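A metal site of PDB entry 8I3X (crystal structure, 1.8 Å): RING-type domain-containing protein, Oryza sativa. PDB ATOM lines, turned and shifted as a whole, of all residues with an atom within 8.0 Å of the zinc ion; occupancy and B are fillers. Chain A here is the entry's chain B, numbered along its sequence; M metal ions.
The zinc ion is bound by ND1 of His 40, SG of Cys 17, SG of Cys 14 and SG of Cys 43.
Merely in contact with the zinc ion: Arg 28 (3.9 Å). Of the 18 residues printed, 5 come within 4 Å of the zinc ion. The nearest printed residue that does not touch the zinc ion is Ile 16 (4.5 Å).
The guanidinium group of Arg 28 lies close to a ring nitrogen (ND1) of His 40. NE2 of His 40 is in hydrogen-bond range of O of Ala 20 (2.9 Å). The side-chain sulfur (SG) of Cys 17 lies close to the backbone NH (N) of Asp 19 (3.5 Å). SG of Cys 14 sits close to N of Ile 16. O of Asp 19 is in hydrogen-bond range of N of Cys 14 (2.7 Å). SG of Cys 43 lies close to NH2 of Arg 28, 3.5 Å away. The side-chain sulfur of Cys 43 lies close to the side-chain carboxylate of Asp 42. The guanidinium group of Arg 28 is in salt-bridge range of the side-chain carboxylate of Asp 42.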
ATOM      1  N   SER A  13      10.082 -31.121   3.786  1.00  0.00           N
ATOM      2  CA  SER A  13       8.684 -31.479   3.592  1.00  0.00           C
ATOM      3  C   SER A  13       7.762 -30.486   4.297  1.00  0.00           C
ATOM      4  O   SER A  13       8.093 -29.941   5.349  1.00  0.00           O
ATOM      5  CB  SER A  13       8.412 -32.901   4.094  1.00  0.00           C
ATOM      6  OG  SER A  13       8.485 -32.971   5.498  1.00  0.00           O
ATOM      7  N   CYS A  14       6.597 -30.256   3.688  1.00  0.00           N
ATOM      8  CA  CYS A  14       5.598 -29.373   4.255  1.00  0.00           C
ATOM      9  C   CYS A  14       4.849 -30.112   5.363  1.00  0.00           C
ATOM     10  O   CYS A  14       4.198 -31.129   5.110  1.00  0.00           O
ATOM     11  CB  CYS A  14       4.635 -28.907   3.160  1.00  0.00           C
ATOM     12  SG  CYS A  14       3.228 -27.895   3.709  1.00  0.00           S
ATOM     13  N   SER A  15       4.935 -29.608   6.591  1.00  0.00           N
ATOM     14  CA  SER A  15       4.265 -30.262   7.711  1.00  0.00           C
ATOM     15  C   SER A  15       2.750 -30.229   7.604  1.00  0.00           C
ATOM     16  O   SER A  15       2.075 -30.927   8.367  1.00  0.00           O
ATOM     17  CB  SER A  15       4.691 -29.609   9.027  1.00  0.00           C
ATOM     18  OG  SER A  15       3.994 -28.386   9.218  1.00  0.00           O
ATOM     19  N   ILE A  16       2.201 -29.437   6.683  1.00  0.00           N
ATOM     20  CA  ILE A  16       0.751 -29.300   6.591  1.00  0.00           C
ATOM     21  C   ILE A  16       0.156 -30.416   5.757  1.00  0.00           C
ATOM     22  O   ILE A  16      -0.824 -31.062   6.147  1.00  0.00           O
ATOM     23  CB  ILE A  16       0.398 -27.911   6.045  1.00  0.00           C
ATOM     24  CG1 ILE A  16       0.838 -26.828   7.034  1.00  0.00           C
ATOM     25  CG2 ILE A  16      -1.083 -27.823   5.753  1.00  0.00           C
ATOM     26  CD1 ILE A  16       0.557 -25.425   6.597  1.00  0.00           C
ATOM     27  N   CYS A  17       0.727 -30.670   4.591  1.00  0.00           N
ATOM     28  CA  CYS A  17       0.243 -31.704   3.695  1.00  0.00           C
ATOM     29  C   CYS A  17       1.175 -32.900   3.628  1.00  0.00           C
ATOM     30  O   CYS A  17       0.842 -33.895   2.967  1.00  0.00           O
ATOM     31  CB  CYS A  17       0.026 -31.129   2.298  1.00  0.00           C
ATOM     32  SG  CYS A  17       1.567 -30.712   1.432  1.00  0.00           S
ATOM     33  N   LEU A  18       2.341 -32.811   4.278  1.00  0.00           N
ATOM     34  CA  LEU A  18       3.341 -33.885   4.355  1.00  0.00           C
ATOM     35  C   LEU A  18       3.974 -34.204   3.010  1.00  0.00           C
ATOM     36  O   LEU A  18       4.595 -35.254   2.852  1.00  0.00           O
ATOM     37  CB  LEU A  18       2.754 -35.150   4.994  1.00  0.00           C
ATOM     38  CG  LEU A  18       2.620 -35.084   6.518  1.00  0.00           C
ATOM     39  CD1 LEU A  18       3.856 -34.436   7.128  1.00  0.00           C
ATOM     40  CD2 LEU A  18       1.378 -34.329   6.950  1.00  0.00           C
ATOM     41  N   ASP A  19       3.850 -33.312   2.029  1.00  0.00           N
ATOM     42  CA  ASP A  19       4.508 -33.459   0.738  1.00  0.00           C
ATOM     43  C   ASP A  19       5.795 -32.645   0.705  1.00  0.00           C
ATOM     44  O   ASP A  19       5.972 -31.676   1.451  1.00  0.00           O
ATOM     45  CB  ASP A  19       3.598 -33.036  -0.407  1.00  0.00           C
ATOM     46  CG  ASP A  19       2.522 -34.045  -0.696  1.00  0.00           C
ATOM     47  OD1 ASP A  19       2.546 -35.128  -0.071  1.00  0.00           O
ATOM     48  OD2 ASP A  19       1.647 -33.752  -1.542  1.00  0.00           O
ATOM     49  N   ALA A  20       6.696 -33.036  -0.187  1.00  0.00           N
ATOM     50  CA  ALA A  20       7.964 -32.337  -0.308  1.00  0.00           C
ATOM     51  C   ALA A  20       7.745 -30.928  -0.848  1.00  0.00           C
ATOM     52  O   ALA A  20       6.950 -30.706  -1.770  1.00  0.00           O
ATOM     53  CB  ALA A  20       8.917 -33.102  -1.227  1.00  0.00           C
ATOM     54  N   VAL A  21       8.446 -29.973  -0.237  1.00  0.00           N
ATOM     55  CA  VAL A  21       8.511 -28.607  -0.746  1.00  0.00           C
ATOM     56  C   VAL A  21       9.705 -28.534  -1.702  1.00  0.00           C
ATOM     57  O   VAL A  21      10.835 -28.791  -1.295  1.00  0.00           O
ATOM     58  CB  VAL A  21       8.667 -27.598   0.394  1.00  0.00           C
ATOM     59  CG1 VAL A  21       8.808 -26.189  -0.147  1.00  0.00           C
ATOM     60  CG2 VAL A  21       7.510 -27.706   1.366  1.00  0.00           C
ATOM     61  N   ARG A  28       4.592 -26.348  -7.623  1.00  0.00           N
ATOM     62  CA  ARG A  28       3.750 -25.676  -6.654  1.00  0.00           C
ATOM     63  C   ARG A  28       4.523 -24.517  -6.042  1.00  0.00           C
ATOM     64  O   ARG A  28       5.733 -24.636  -5.808  1.00  0.00           O
ATOM     65  CB  ARG A  28       3.306 -26.629  -5.519  1.00  0.00           C
ATOM     66  CG  ARG A  28       2.249 -27.655  -5.893  1.00  0.00           C
ATOM     67  CD  ARG A  28       1.992 -28.590  -4.715  1.00  0.00           C
ATOM     68  NE  ARG A  28       1.200 -27.953  -3.658  1.00  0.00           N
ATOM     69  CZ  ARG A  28       0.907 -28.519  -2.494  1.00  0.00           C
ATOM     70  NH1 ARG A  28       1.342 -29.741  -2.221  1.00  0.00           N
ATOM     71  NH2 ARG A  28       0.174 -27.855  -1.607  1.00  0.00           N
ATOM     72  N   SER A  29       3.828 -23.416  -5.782  1.00  0.00           N
ATOM     73  CA  SER A  29       4.469 -22.271  -5.168  1.00  0.00           C
ATOM     74  C   SER A  29       4.879 -22.602  -3.736  1.00  0.00           C
ATOM     75  O   SER A  29       4.278 -23.467  -3.076  1.00  0.00           O
ATOM     76  CB  SER A  29       3.532 -21.060  -5.176  1.00  0.00           C
ATOM     77  OG  SER A  29       3.201 -20.720  -6.511  1.00  0.00           O
ATOM     78  N   GLU A  38       9.537 -24.098   6.062  1.00  0.00           N
ATOM     79  CA  GLU A  38       9.077 -23.968   4.698  1.00  0.00           C
ATOM     80  C   GLU A  38       7.813 -24.774   4.455  1.00  0.00           C
ATOM     81  O   GLU A  38       7.574 -25.801   5.096  1.00  0.00           O
ATOM     82  CB  GLU A  38      10.159 -24.416   3.712  1.00  0.00           C
ATOM     83  CG  GLU A  38      11.467 -23.670   3.882  1.00  0.00           C
ATOM     84  CD  GLU A  38      12.534 -24.196   2.949  1.00  0.00           C
ATOM     85  OE1 GLU A  38      12.304 -24.195   1.727  1.00  0.00           O
ATOM     86  OE2 GLU A  38      13.608 -24.610   3.457  1.00  0.00           O
ATOM     87  N   PHE A  39       7.023 -24.293   3.514  1.00  0.00           N
ATOM     88  CA  PHE A  39       5.688 -24.805   3.249  1.00  0.00           C
ATOM     89  C   PHE A  39       5.364 -24.562   1.792  1.00  0.00           C
ATOM     90  O   PHE A  39       5.980 -23.731   1.127  1.00  0.00           O
ATOM     91  CB  PHE A  39       4.644 -24.121   4.130  1.00  0.00           C
ATOM     92  CG  PHE A  39       4.942 -24.189   5.604  1.00  0.00           C
ATOM     93  CD1 PHE A  39       4.522 -25.272   6.361  1.00  0.00           C
ATOM     94  CD2 PHE A  39       5.639 -23.172   6.234  1.00  0.00           C
ATOM     95  CE1 PHE A  39       4.794 -25.339   7.712  1.00  0.00           C
ATOM     96  CE2 PHE A  39       5.920 -23.237   7.580  1.00  0.00           C
ATOM     97  CZ  PHE A  39       5.494 -24.319   8.325  1.00  0.00           C
ATOM     98  N   HIS A  40       4.363 -25.280   1.291  1.00  0.00           N
ATOM     99  CA  HIS A  40       3.736 -24.846   0.058  1.00  0.00           C
ATOM    100  C   HIS A  40       2.941 -23.575   0.323  1.00  0.00           C
ATOM    101  O   HIS A  40       2.402 -23.376   1.417  1.00  0.00           O
ATOM    102  CB  HIS A  40       2.816 -25.930  -0.499  1.00  0.00           C
ATOM    103  CG  HIS A  40       3.520 -27.225  -0.729  1.00  0.00           C
ATOM    104  ND1 HIS A  40       3.407 -28.297   0.130  1.00  0.00           N
ATOM    105  CD2 HIS A  40       4.365 -27.611  -1.711  1.00  0.00           C
ATOM    106  CE1 HIS A  40       4.155 -29.288  -0.325  1.00  0.00           C
ATOM    107  NE2 HIS A  40       4.746 -28.897  -1.437  1.00  0.00           N
ATOM    108  N   LEU A  41       2.879 -22.702  -0.676  1.00  0.00           N
ATOM    109  CA  LEU A  41       2.203 -21.418  -0.487  1.00  0.00           C
ATOM    110  C   LEU A  41       0.729 -21.604  -0.110  1.00  0.00           C
ATOM    111  O   LEU A  41       0.243 -20.944   0.818  1.00  0.00           O
ATOM    112  CB  LEU A  41       2.330 -20.549  -1.728  1.00  0.00           C
ATOM    113  CG  LEU A  41       1.706 -19.157  -1.573  1.00  0.00           C
ATOM    114  CD1 LEU A  41       2.221 -18.472  -0.338  1.00  0.00           C
ATOM    115  CD2 LEU A  41       2.031 -18.332  -2.819  1.00  0.00           C
ATOM    116  N   ASP A  42       0.003 -22.472  -0.807  1.00  0.00           N
ATOM    117  CA  ASP A  42      -1.433 -22.567  -0.500  1.00  0.00           C
ATOM    118  C   ASP A  42      -1.660 -23.224   0.857  1.00  0.00           C
ATOM    119  O   ASP A  42      -2.624 -22.884   1.549  1.00  0.00           O
ATOM    120  CB  ASP A  42      -2.199 -23.277  -1.633  1.00  0.00           C
ATOM    121  CG  ASP A  42      -1.678 -24.684  -1.938  1.00  0.00           C
ATOM    122  OD1 ASP A  42      -0.684 -25.127  -1.329  1.00  0.00           O
ATOM    123  OD2 ASP A  42      -2.286 -25.336  -2.816  1.00  0.00           O
ATOM    124  N   CYS A  43      -0.790 -24.146   1.265  1.00  0.00           N
ATOM    125  CA  CYS A  43      -0.910 -24.728   2.595  1.00  0.00           C
ATOM    126  C   CYS A  43      -0.787 -23.676   3.686  1.00  0.00           C
ATOM    127  O   CYS A  43      -1.688 -23.521   4.526  1.00  0.00           O
ATOM    128  CB  CYS A  43       0.164 -25.801   2.778  1.00  0.00           C
ATOM    129  SG  CYS A  43      -0.152 -27.233   1.784  1.00  0.00           S
ATOM    130  N   ILE A  44       0.329 -22.955   3.703  1.00  0.00           N
ATOM    131  CA  ILE A  44       0.570 -22.017   4.804  1.00  0.00           C
ATOM    132  C   ILE A  44      -0.373 -20.825   4.708  1.00  0.00           C
ATOM    133  O   ILE A  44      -0.809 -20.283   5.736  1.00  0.00           O
ATOM    134  CB  ILE A  44       2.052 -21.579   4.830  1.00  0.00           C
ATOM    135  CG1 ILE A  44       2.396 -20.900   6.152  1.00  0.00           C
ATOM    136  CG2 ILE A  44       2.382 -20.670   3.675  1.00  0.00           C
ATOM    137  CD1 ILE A  44       2.323 -21.826   7.341  1.00  0.00           C
HETATM  138 ZN    ZN M   1       1.907 -28.437   1.826  1.00  0.00          ZN
